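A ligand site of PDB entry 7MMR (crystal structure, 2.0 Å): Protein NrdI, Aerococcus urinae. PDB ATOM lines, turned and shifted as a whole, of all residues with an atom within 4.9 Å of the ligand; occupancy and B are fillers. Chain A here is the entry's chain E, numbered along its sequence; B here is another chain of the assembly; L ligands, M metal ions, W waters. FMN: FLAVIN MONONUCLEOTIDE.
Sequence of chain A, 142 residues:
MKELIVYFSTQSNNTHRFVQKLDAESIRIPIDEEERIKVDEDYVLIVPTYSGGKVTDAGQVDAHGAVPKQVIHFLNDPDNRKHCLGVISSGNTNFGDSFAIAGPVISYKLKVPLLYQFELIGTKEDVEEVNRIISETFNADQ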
ATOM      1  N   PHE A   8       7.279 -18.150 -15.739  1.00  0.00           N
ATOM      2  CA  PHE A   8       6.666 -19.240 -14.949  1.00  0.00           C
ATOM      3  C   PHE A   8       5.905 -20.166 -15.895  1.00  0.00           C
ATOM      4  O   PHE A   8       5.309 -19.681 -16.884  1.00  0.00           O
ATOM      5  CB  PHE A   8       5.741 -18.700 -13.850  1.00  0.00           C
ATOM      6  CG  PHE A   8       5.035 -19.776 -13.079  1.00  0.00           C
ATOM      7  CD1 PHE A   8       5.673 -20.424 -12.023  1.00  0.00           C
ATOM      8  CD2 PHE A   8       3.758 -20.193 -13.420  1.00  0.00           C
ATOM      9  CE1 PHE A   8       5.037 -21.440 -11.322  1.00  0.00           C
ATOM     10  CE2 PHE A   8       3.119 -21.197 -12.713  1.00  0.00           C
ATOM     11  CZ  PHE A   8       3.766 -21.827 -11.671  1.00  0.00           C
ATOM     12  N   SER A   9       5.947 -21.464 -15.598  1.00  0.00           N
ATOM     13  CA  SER A   9       5.218 -22.536 -16.325  1.00  0.00           C
ATOM     14  C   SER A   9       4.869 -23.637 -15.328  1.00  0.00           C
ATOM     15  O   SER A   9       5.755 -24.018 -14.534  1.00  0.00           O
ATOM     16  CB  SER A   9       6.053 -23.053 -17.478  1.00  0.00           C
ATOM     17  OG  SER A   9       5.256 -23.786 -18.405  1.00  0.00           O
ATOM     18  N   THR A  10       3.623 -24.106 -15.320  1.00  0.00           N
ATOM     19  CA  THR A  10       3.173 -25.237 -14.468  1.00  0.00           C
ATOM     20  C   THR A  10       3.717 -26.531 -15.084  1.00  0.00           C
ATOM     21  O   THR A  10       4.536 -26.451 -16.030  1.00  0.00           O
ATOM     22  CB  THR A  10       1.641 -25.281 -14.310  1.00  0.00           C
ATOM     23  OG1 THR A  10       1.086 -25.674 -15.564  1.00  0.00           O
ATOM     24  CG2 THR A  10       1.059 -23.967 -13.844  1.00  0.00           C
ATOM     25  N   SER A  12       2.394 -28.530 -17.057  1.00  0.00           N
ATOM     26  CA  SER A  12       1.959 -28.676 -18.483  1.00  0.00           C
ATOM     27  C   SER A  12       3.008 -28.094 -19.449  1.00  0.00           C
ATOM     28  O   SER A  12       3.023 -28.534 -20.604  1.00  0.00           O
ATOM     29  CB  SER A  12       0.583 -28.084 -18.715  1.00  0.00           C
ATOM     30  OG  SER A  12       0.422 -26.841 -18.062  1.00  0.00           O
ATOM     31  N   ASN A  13       3.843 -27.158 -18.990  1.00  0.00           N
ATOM     32  CA  ASN A  13       5.066 -26.687 -19.691  1.00  0.00           C
ATOM     33  C   ASN A  13       4.730 -26.004 -21.025  1.00  0.00           C
ATOM     34  O   ASN A  13       5.599 -26.015 -21.914  1.00  0.00           O
ATOM     35  CB  ASN A  13       6.055 -27.844 -19.946  1.00  0.00           C
ATOM     36  CG  ASN A  13       6.905 -28.175 -18.728  1.00  0.00           C
ATOM     37  OD1 ASN A  13       7.394 -27.277 -18.041  1.00  0.00           O
ATOM     38  ND2 ASN A  13       7.092 -29.457 -18.476  1.00  0.00           N
ATOM     39  N   ASN A  14       3.544 -25.394 -21.156  1.00  0.00           N
ATOM     40  CA  ASN A  14       3.142 -24.643 -22.384  1.00  0.00           C
ATOM     41  C   ASN A  14       4.017 -23.383 -22.505  1.00  0.00           C
ATOM     42  O   ASN A  14       4.595 -23.181 -23.592  1.00  0.00           O
ATOM     43  CB  ASN A  14       1.670 -24.232 -22.385  1.00  0.00           C
ATOM     44  CG  ASN A  14       0.716 -25.389 -22.627  1.00  0.00           C
ATOM     45  OD1 ASN A  14       1.125 -26.520 -22.849  1.00  0.00           O
ATOM     46  ND2 ASN A  14      -0.575 -25.094 -22.605  1.00  0.00           N
ATOM     47  N   THR A  15       4.082 -22.581 -21.447  1.00  0.00           N
ATOM     48  CA  THR A  15       4.839 -21.297 -21.383  1.00  0.00           C
ATOM     49  C   THR A  15       6.335 -21.587 -21.510  1.00  0.00           C
ATOM     50  O   THR A  15       7.020 -20.836 -22.227  1.00  0.00           O
ATOM     51  CB  THR A  15       4.504 -20.519 -20.099  1.00  0.00           C
ATOM     52  OG1 THR A  15       3.084 -20.492 -19.964  1.00  0.00           O
ATOM     53  CG2 THR A  15       5.044 -19.110 -20.110  1.00  0.00           C
ATOM     54  N   HIS A  16       6.816 -22.652 -20.850  1.00  0.00           N
ATOM     55  CA  HIS A  16       8.220 -23.135 -20.944  1.00  0.00           C
ATOM     56  C   HIS A  16       8.587 -23.335 -22.420  1.00  0.00           C
ATOM     57  O   HIS A  16       9.611 -22.782 -22.851  1.00  0.00           O
ATOM     58  CB  HIS A  16       8.423 -24.417 -20.117  1.00  0.00           C
ATOM     59  CG  HIS A  16       9.723 -25.088 -20.351  1.00  0.00           C
ATOM     60  ND1 HIS A  16      10.908 -24.634 -19.793  1.00  0.00           N
ATOM     61  CD2 HIS A  16      10.051 -26.179 -21.096  1.00  0.00           C
ATOM     62  CE1 HIS A  16      11.906 -25.416 -20.171  1.00  0.00           C
ATOM     63  NE2 HIS A  16      11.398 -26.365 -20.973  1.00  0.00           N
ATOM     64  N   PRO A  48       1.621 -17.469 -17.541  1.00  0.00           N
ATOM     65  CA  PRO A  48       0.263 -17.881 -17.897  1.00  0.00           C
ATOM     66  C   PRO A  48      -0.782 -17.433 -16.865  1.00  0.00           C
ATOM     67  O   PRO A  48      -0.393 -17.033 -15.778  1.00  0.00           O
ATOM     68  CB  PRO A  48       0.392 -19.409 -17.918  1.00  0.00           C
ATOM     69  CG  PRO A  48       1.364 -19.687 -16.781  1.00  0.00           C
ATOM     70  CD  PRO A  48       2.342 -18.537 -16.830  1.00  0.00           C
ATOM     71  N   THR A  49      -2.067 -17.498 -17.230  1.00  0.00           N
ATOM     72  CA  THR A  49      -3.213 -17.037 -16.408  1.00  0.00           C
ATOM     73  C   THR A  49      -3.968 -18.259 -15.866  1.00  0.00           C
ATOM     74  O   THR A  49      -4.184 -19.202 -16.641  1.00  0.00           O
ATOM     75  CB  THR A  49      -4.130 -16.116 -17.224  1.00  0.00           C
ATOM     76  OG1 THR A  49      -3.304 -15.071 -17.753  1.00  0.00           O
ATOM     77  CG2 THR A  49      -5.257 -15.527 -16.406  1.00  0.00           C
ATOM     78  N   TYR A  50      -4.365 -18.224 -14.588  1.00  0.00           N
ATOM     79  CA  TYR A  50      -4.977 -19.383 -13.881  1.00  0.00           C
ATOM     80  C   TYR A  50      -6.162 -18.956 -13.014  1.00  0.00           C
ATOM     81  O   TYR A  50      -6.436 -19.626 -11.998  1.00  0.00           O
ATOM     82  CB  TYR A  50      -3.889 -20.136 -13.110  1.00  0.00           C
ATOM     83  CG  TYR A  50      -3.164 -21.153 -13.959  1.00  0.00           C
ATOM     84  CD1 TYR A  50      -3.733 -22.382 -14.231  1.00  0.00           C
ATOM     85  CD2 TYR A  50      -1.933 -20.870 -14.527  1.00  0.00           C
ATOM     86  CE1 TYR A  50      -3.090 -23.317 -15.023  1.00  0.00           C
ATOM     87  CE2 TYR A  50      -1.281 -21.794 -15.322  1.00  0.00           C
ATOM     88  CZ  TYR A  50      -1.854 -23.018 -15.574  1.00  0.00           C
ATOM     89  OH  TYR A  50      -1.224 -23.940 -16.353  1.00  0.00           O
ATOM     90  N   SER A  51      -6.896 -17.902 -13.406  1.00  0.00           N
ATOM     91  CA  SER A  51      -8.139 -17.451 -12.703  1.00  0.00           C
ATOM     92  C   SER A  51      -9.291 -18.424 -13.012  1.00  0.00           C
ATOM     93  O   SER A  51     -10.221 -18.494 -12.184  1.00  0.00           O
ATOM     94  CB  SER A  51      -8.492 -16.034 -13.056  1.00  0.00           C
ATOM     95  OG  SER A  51      -8.547 -15.857 -14.464  1.00  0.00           O
ATOM     96  N   GLY A  52      -9.234 -19.118 -14.147  1.00  0.00           N
ATOM     97  CA  GLY A  52     -10.223 -20.148 -14.538  1.00  0.00           C
ATOM     98  C   GLY A  52     -11.561 -19.544 -14.947  1.00  0.00           C
ATOM     99  O   GLY A  52     -12.575 -20.267 -14.875  1.00  0.00           O
ATOM    100  N   GLY A  53     -11.561 -18.283 -15.373  1.00  0.00           N
ATOM    101  CA  GLY A  53     -12.763 -17.575 -15.876  1.00  0.00           C
ATOM    102  C   GLY A  53     -13.780 -17.331 -14.765  1.00  0.00           C
ATOM    103  O   GLY A  53     -14.981 -17.272 -15.080  1.00  0.00           O
ATOM    104  N   SER A  90      -0.045 -15.117 -21.089  1.00  0.00           N
ATOM    105  CA  SER A  90      -0.628 -16.167 -21.968  1.00  0.00           C
ATOM    106  C   SER A  90      -1.901 -16.720 -21.335  1.00  0.00           C
ATOM    107  O   SER A  90      -2.168 -16.440 -20.142  1.00  0.00           O
ATOM    108  CB  SER A  90       0.363 -17.258 -22.253  1.00  0.00           C
ATOM    109  OG  SER A  90       0.588 -18.053 -21.115  1.00  0.00           O
ATOM    110  N   GLY A  91      -2.647 -17.477 -22.129  1.00  0.00           N
ATOM    111  CA  GLY A  91      -3.871 -18.168 -21.711  1.00  0.00           C
ATOM    112  C   GLY A  91      -4.579 -18.765 -22.908  1.00  0.00           C
ATOM    113  O   GLY A  91      -3.890 -19.335 -23.772  1.00  0.00           O
ATOM    114  N   ASN A  92      -5.898 -18.607 -22.965  1.00  0.00           N
ATOM    115  CA  ASN A  92      -6.761 -19.171 -24.028  1.00  0.00           C
ATOM    116  C   ASN A  92      -7.990 -18.267 -24.150  1.00  0.00           C
ATOM    117  O   ASN A  92      -8.656 -18.054 -23.120  1.00  0.00           O
ATOM    118  CB  ASN A  92      -7.123 -20.624 -23.710  1.00  0.00           C
ATOM    119  CG  ASN A  92      -7.704 -21.373 -24.902  1.00  0.00           C
ATOM    120  OD1 ASN A  92      -8.586 -20.857 -25.578  1.00  0.00           O
ATOM    121  ND2 ASN A  92      -7.217 -22.576 -25.153  1.00  0.00           N
ATOM    122  N   PHE A  95     -11.528 -18.505 -22.500  1.00  0.00           N
ATOM    123  CA  PHE A  95     -11.815 -17.998 -21.125  1.00  0.00           C
ATOM    124  C   PHE A  95     -12.442 -16.593 -21.203  1.00  0.00           C
ATOM    125  O   PHE A  95     -12.738 -16.015 -20.127  1.00  0.00           O
ATOM    126  CB  PHE A  95     -10.563 -18.006 -20.256  1.00  0.00           C
ATOM    127  CG  PHE A  95     -10.226 -19.356 -19.693  1.00  0.00           C
ATOM    128  CD1 PHE A  95     -10.924 -19.861 -18.608  1.00  0.00           C
ATOM    129  CD2 PHE A  95      -9.235 -20.141 -20.272  1.00  0.00           C
ATOM    130  CE1 PHE A  95     -10.628 -21.119 -18.101  1.00  0.00           C
ATOM    131  CE2 PHE A  95      -8.948 -21.400 -19.766  1.00  0.00           C
ATOM    132  CZ  PHE A  95      -9.631 -21.880 -18.676  1.00  0.00           C
ATOM    133  N   SER A  98     -11.689 -13.162 -19.222  1.00  0.00           N
ATOM    134  CA  SER A  98     -10.580 -13.597 -18.332  1.00  0.00           C
ATOM    135  C   SER A  98      -9.333 -13.998 -19.144  1.00  0.00           C
ATOM    136  O   SER A  98      -8.370 -14.476 -18.519  1.00  0.00           O
ATOM    137  CB  SER A  98     -11.026 -14.721 -17.428  1.00  0.00           C
ATOM    138  OG  SER A  98     -11.900 -14.236 -16.420  1.00  0.00           O
ATOM    139  N   PHE A  99      -9.341 -13.796 -20.467  1.00  0.00           N
ATOM    140  CA  PHE A  99      -8.209 -14.195 -21.352  1.00  0.00           C
ATOM    141  C   PHE A  99      -6.950 -13.415 -20.965  1.00  0.00           C
ATOM    142  O   PHE A  99      -6.964 -12.174 -21.060  1.00  0.00           O
ATOM    143  CB  PHE A  99      -8.530 -13.970 -22.829  1.00  0.00           C
ATOM    144  CG  PHE A  99      -7.309 -14.006 -23.715  1.00  0.00           C
ATOM    145  CD1 PHE A  99      -6.504 -15.129 -23.756  1.00  0.00           C
ATOM    146  CD2 PHE A  99      -6.947 -12.901 -24.478  1.00  0.00           C
ATOM    147  CE1 PHE A  99      -5.363 -15.170 -24.559  1.00  0.00           C
ATOM    148  CE2 PHE A  99      -5.816 -12.943 -25.281  1.00  0.00           C
ATOM    149  CZ  PHE A  99      -5.021 -14.074 -25.312  1.00  0.00           C
ATOM    150  N   ALA A 100      -5.899 -14.134 -20.560  1.00  0.00           N
ATOM    151  CA  ALA A 100      -4.506 -13.641 -20.360  1.00  0.00           C
ATOM    152  C   ALA A 100      -4.445 -12.509 -19.329  1.00  0.00           C
ATOM    153  O   ALA A 100      -3.485 -11.715 -19.389  1.00  0.00           O
ATOM    154  CB  ALA A 100      -3.942 -13.203 -21.691  1.00  0.00           C
ATOM    155  N   LEU A 120      -1.181 -20.684 -25.279  1.00  0.00           N
ATOM    156  CA  LEU A 120      -0.591 -22.045 -25.210  1.00  0.00           C
ATOM    157  C   LEU A 120       0.908 -21.961 -25.492  1.00  0.00           C
ATOM    158  O   LEU A 120       1.591 -21.205 -24.772  1.00  0.00           O
ATOM    159  CB  LEU A 120      -1.351 -22.951 -26.194  1.00  0.00           C
ATOM    160  CG  LEU A 120      -2.873 -22.936 -26.051  1.00  0.00           C
ATOM    161  CD1 LEU A 120      -3.524 -23.864 -27.053  1.00  0.00           C
ATOM    162  CD2 LEU A 120      -3.297 -23.295 -24.637  1.00  0.00           C
ATOM    163  N   LYS B  36      -1.476 -31.076 -10.980  1.00  0.00           N
ATOM    164  CA  LYS B  36      -2.285 -30.565 -12.118  1.00  0.00           C
ATOM    165  C   LYS B  36      -3.718 -31.127 -12.028  1.00  0.00           C
ATOM    166  O   LYS B  36      -4.649 -30.375 -12.382  1.00  0.00           O
ATOM    167  CB  LYS B  36      -1.620 -30.921 -13.454  1.00  0.00           C
ATOM    168  CG  LYS B  36      -2.343 -30.422 -14.702  1.00  0.00           C
ATOM    169  CD  LYS B  36      -2.529 -28.920 -14.767  1.00  0.00           C
ATOM    170  CE  LYS B  36      -1.241 -28.151 -14.976  1.00  0.00           C
ATOM    171  NZ  LYS B  36      -1.509 -26.739 -15.346  1.00  0.00           N
ATOM    172  N   GLU B  39      -5.547 -29.002  -9.404  1.00  0.00           N
ATOM    173  CA  GLU B  39      -5.771 -27.696 -10.083  1.00  0.00           C
ATOM    174  C   GLU B  39      -7.037 -27.783 -10.946  1.00  0.00           C
ATOM    175  O   GLU B  39      -7.923 -26.913 -10.799  1.00  0.00           O
ATOM    176  CB  GLU B  39      -4.525 -27.336 -10.905  1.00  0.00           C
ATOM    177  CG  GLU B  39      -4.565 -25.955 -11.534  1.00  0.00           C
ATOM    178  CD  GLU B  39      -3.218 -25.384 -11.948  1.00  0.00           C
ATOM    179  OE1 GLU B  39      -2.854 -24.291 -11.458  1.00  0.00           O
ATOM    180  OE2 GLU B  39      -2.520 -26.033 -12.766  1.00  0.00           O
ATOM    181  N   VAL B  40      -7.138 -28.808 -11.794  1.00  0.00           N
ATOM    182  CA  VAL B  40      -8.264 -28.977 -12.768  1.00  0.00           C
ATOM    183  C   VAL B  40      -9.545 -29.330 -12.007  1.00  0.00           C
ATOM    184  O   VAL B  40     -10.587 -28.687 -12.293  1.00  0.00           O
ATOM    185  CB  VAL B  40      -7.917 -30.024 -13.841  1.00  0.00           C
ATOM    186  CG1 VAL B  40      -9.129 -30.433 -14.671  1.00  0.00           C
ATOM    187  CG2 VAL B  40      -6.808 -29.520 -14.751  1.00  0.00           C
ATOM    188  N   ARG B  43     -11.061 -26.284 -10.236  1.00  0.00           N
ATOM    189  CA  ARG B  43     -11.603 -25.267 -11.176  1.00  0.00           C
ATOM    190  C   ARG B  43     -12.943 -25.751 -11.762  1.00  0.00           C
ATOM    191  O   ARG B  43     -13.906 -24.965 -11.707  1.00  0.00           O
ATOM    192  CB  ARG B  43     -10.592 -24.911 -12.269  1.00  0.00           C
ATOM    193  CG  ARG B  43     -11.060 -23.830 -13.239  1.00  0.00           C
ATOM    194  CD  ARG B  43     -11.828 -22.688 -12.572  1.00  0.00           C
ATOM    195  NE  ARG B  43     -11.108 -22.111 -11.441  1.00  0.00           N
ATOM    196  CZ  ARG B  43     -11.676 -21.462 -10.421  1.00  0.00           C
ATOM    197  NH1 ARG B  43     -12.988 -21.300 -10.373  1.00  0.00           N
ATOM    198  NH2 ARG B  43     -10.918 -20.996  -9.452  1.00  0.00           N
ATOM    199  N   ILE B 212     -11.017 -26.263 -20.706  1.00  0.00           N
ATOM    200  CA  ILE B 212     -10.314 -27.092 -19.679  1.00  0.00           C
ATOM    201  C   ILE B 212     -10.353 -28.564 -20.105  1.00  0.00           C
ATOM    202  O   ILE B 212      -9.323 -29.244 -19.926  1.00  0.00           O
ATOM    203  CB  ILE B 212     -10.921 -26.867 -18.282  1.00  0.00           C
ATOM    204  CG1 ILE B 212     -10.698 -25.426 -17.805  1.00  0.00           C
ATOM    205  CG2 ILE B 212     -10.364 -27.885 -17.286  1.00  0.00           C
ATOM    206  CD1 ILE B 212     -11.234 -25.134 -16.428  1.00  0.00           C
ATOM    207  N   PHE B 215      -7.719 -28.940 -22.820  1.00  0.00           N
ATOM    208  CA  PHE B 215      -6.400 -28.787 -22.169  1.00  0.00           C
ATOM    209  C   PHE B 215      -6.023 -30.106 -21.461  1.00  0.00           C
ATOM    210  O   PHE B 215      -4.893 -30.595 -21.652  1.00  0.00           O
ATOM    211  CB  PHE B 215      -6.391 -27.651 -21.138  1.00  0.00           C
ATOM    212  CG  PHE B 215      -5.243 -27.778 -20.166  1.00  0.00           C
ATOM    213  CD1 PHE B 215      -3.985 -27.284 -20.487  1.00  0.00           C
ATOM    214  CD2 PHE B 215      -5.408 -28.434 -18.956  1.00  0.00           C
ATOM    215  CE1 PHE B 215      -2.927 -27.429 -19.598  1.00  0.00           C
ATOM    216  CE2 PHE B 215      -4.348 -28.581 -18.077  1.00  0.00           C
ATOM    217  CZ  PHE B 215      -3.113 -28.078 -18.393  1.00  0.00           C
ATOM    218  N   ASN B 282      -2.309 -27.920 -27.762  1.00  0.00           N
ATOM    219  CA  ASN B 282      -2.598 -28.572 -26.457  1.00  0.00           C
ATOM    220  C   ASN B 282      -2.332 -30.089 -26.533  1.00  0.00           C
ATOM    221  O   ASN B 282      -2.399 -30.739 -25.478  1.00  0.00           O
ATOM    222  CB  ASN B 282      -4.001 -28.249 -25.944  1.00  0.00           C
ATOM    223  CG  ASN B 282      -4.010 -27.083 -24.978  1.00  0.00           C
ATOM    224  OD1 ASN B 282      -2.975 -26.691 -24.447  1.00  0.00           O
ATOM    225  ND2 ASN B 282      -5.180 -26.518 -24.732  1.00  0.00           N
HETATM  226  N1  FMN L   1      -6.271 -18.900 -19.593  1.00  0.00           N
HETATM  227  C2  FMN L   1      -6.738 -17.628 -19.529  1.00  0.00           C
HETATM  228  O2  FMN L   1      -6.487 -16.875 -20.479  1.00  0.00           O
HETATM  229  N3  FMN L   1      -7.451 -17.159 -18.479  1.00  0.00           N
HETATM  230  C4  FMN L   1      -7.752 -17.928 -17.427  1.00  0.00           C
HETATM  231  O4  FMN L   1      -8.421 -17.474 -16.470  1.00  0.00           O
HETATM  232  C4A FMN L   1      -7.289 -19.340 -17.427  1.00  0.00           C
HETATM  233  N5  FMN L   1      -7.540 -20.196 -16.403  1.00  0.00           N
HETATM  234  C5A FMN L   1      -7.106 -21.481 -16.426  1.00  0.00           C
HETATM  235  C6  FMN L   1      -7.397 -22.318 -15.362  1.00  0.00           C
HETATM  236  C7  FMN L   1      -6.969 -23.640 -15.364  1.00  0.00           C
HETATM  237  C7M FMN L   1      -7.302 -24.534 -14.194  1.00  0.00           C
HETATM  238  C8  FMN L   1      -6.184 -24.162 -16.513  1.00  0.00           C
HETATM  239  C8M FMN L   1      -5.693 -25.591 -16.546  1.00  0.00           C
HETATM  240  C9  FMN L   1      -5.884 -23.323 -17.576  1.00  0.00           C
HETATM  241  C9A FMN L   1      -6.321 -21.997 -17.588  1.00  0.00           C
HETATM  242  N10 FMN L   1      -6.028 -21.110 -18.666  1.00  0.00           N
HETATM  243  C10 FMN L   1      -6.504 -19.785 -18.600  1.00  0.00           C
HETATM  244  C1' FMN L   1      -5.247 -21.550 -19.820  1.00  0.00           C
HETATM  245  C2' FMN L   1      -3.761 -21.629 -19.462  1.00  0.00           C
HETATM  246  O2' FMN L   1      -3.257 -20.338 -19.073  1.00  0.00           O
HETATM  247  C3' FMN L   1      -2.967 -22.182 -20.643  1.00  0.00           C
HETATM  248  O3' FMN L   1      -3.259 -23.579 -20.764  1.00  0.00           O
HETATM  249  C4' FMN L   1      -1.456 -21.964 -20.520  1.00  0.00           C
HETATM  250  O4' FMN L   1      -0.848 -22.283 -21.782  1.00  0.00           O
HETATM  251  C5' FMN L   1      -0.844 -22.796 -19.401  1.00  0.00           C
HETATM  252  O5' FMN L   1       0.551 -22.498 -19.279  1.00  0.00           O
HETATM  253  P   FMN L   1       1.583 -23.495 -18.548  1.00  0.00           P
HETATM  254  O1P FMN L   1       1.180 -23.533 -17.101  1.00  0.00           O
HETATM  255  O2P FMN L   1       2.935 -22.834 -18.788  1.00  0.00           O
HETATM  256  O3P FMN L   1       1.459 -24.820 -19.266  1.00  0.00           O
HETATM  257 CA    CA M   1      -5.922 -24.003 -22.383  1.00  0.00          CA
HETATM  258  O   HOH W   1       1.271 -20.572 -22.223  1.00  0.00           O
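The side-chain hydroxyl (OG) of Ser 9 lies within hydrogen-bond range of the backbone NH (N) of Thr 15 (3.5 Å). The side-chain hydroxyl (OH) of Tyr 50 is in hydrogen-bond range of the side-chain hydroxyl (OG1) of Thr 10 (3.0 Å). The side-chain amino group of Lys 36 of chain B lies within hydrogen-bond range of the side-chain hydroxyl of Tyr 50 (3.0 Å). OG1 of Thr 10 sits at hydrogen-bond distance from OG of Ser 12 (2.8 Å). The side-chain hydroxyl of Ser 12 sits at hydrogen-bond distance from the side-chain amino group of Lys 36 of chain B (3.3 Å). OG1 of Thr 10 is in hydrogen-bond range of NZ of Lys 36 of chain B (2.8 Å). OG1 of Thr 49 is in hydrogen-bond range of O of Ser 90 (3.0 Å). OD1 of Asn 282 of chain B is in hydrogen-bond range of ND2 of Asn 14, 3.4 Å away.
The side-chain hydroxyl (OG) of Ser 9 lies within hydrogen-bond range of an oxygen (O2P) of the ligand (2.5 Å). The side-chain hydroxyl (OH) of Tyr 50 sits at hydrogen-bond distance from an oxygen (O1P) of the ligand. O3P of the ligand lies within hydrogen-bond range of OG of Ser 12 (2.6 Å). N of Ser 51 sits at hydrogen-bond distance from O4 of the ligand (3.4 Å). An oxygen (O4) of the ligand is in hydrogen-bond range of the side-chain hydroxyl (OG) of Ser 51. N of Thr 15 is in hydrogen-bond range of O2P of the ligand. The side-chain hydroxyl (OG1) of Thr 15 is in hydrogen-bond range of an oxygen (O2P) of the ligand (2.6 Å). An oxygen (O1P) of the ligand lies within hydrogen-bond range of the backbone NH (N) of Thr 10. OG1 of Thr 10 is in hydrogen-bond range of O1P of the ligand. An oxygen (O2) of the ligand sits at hydrogen-bond distance from the backbone NH of Ala 100 (2.8 Å). The backbone carbonyl oxygen (O) of Ser 98 is in hydrogen-bond range of a nitrogen (N3) of the ligand, at 2.8 Å. The backbone carbonyl oxygen (O) of Thr 49 lies within hydrogen-bond range of an oxygen (O2') of the ligand. N of Asn 14 lies within hydrogen-bond range of O3P of the ligand, at 2.9 Å. ND2 of Asn 14 lies within hydrogen-bond range of O4' of the ligand. The backbone NH of Gly 52 sits at hydrogen-bond distance from an oxygen (O4) of the ligand, 3.0 Å away. The backbone NH (N) of Asn 92 is in hydrogen-bond range of an oxygen (O2) of the ligand (3.1 Å). The backbone NH (N) of Asn 13 sits at hydrogen-bond distance from an oxygen (O3P) of the ligand (3.4 Å). The backbone NH of Gly 53 is in hydrogen-bond range of an oxygen (O4) of the ligand, at 3.4 Å.
Residues that only touch the ligand: Pro 48 (3.4 Å), Gly 91 (3.2 Å), Phe 95 (3.1 Å), Phe 99 (3.3 Å), Leu 120 (3.4 Å), Arg 43 of chain B (3.8 Å) and Phe 215 of chain B (3.6 Å). Hydrophobic or aromatic side chains within 4 Å of the ligand: Pro 48, Tyr 50, Phe 95, Phe 99, Leu 120 and Phe 215 of chain B. Of the 29 residues printed, 21 come within 4 Å of the ligand. Along chain A the residues within 4 Å of the ligand span positions 9 to 120.
Water W1 lies within hydrogen-bond range of the backbone carbonyl oxygen (O) of Leu 120 (2.6 Å), an oxygen (O4') of the ligand (2.8 Å), the side-chain hydroxyl (OG) of Ser 90 (2.8 Å) and the side-chain hydroxyl (OG1) of Thr 15 (2.9 Å).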
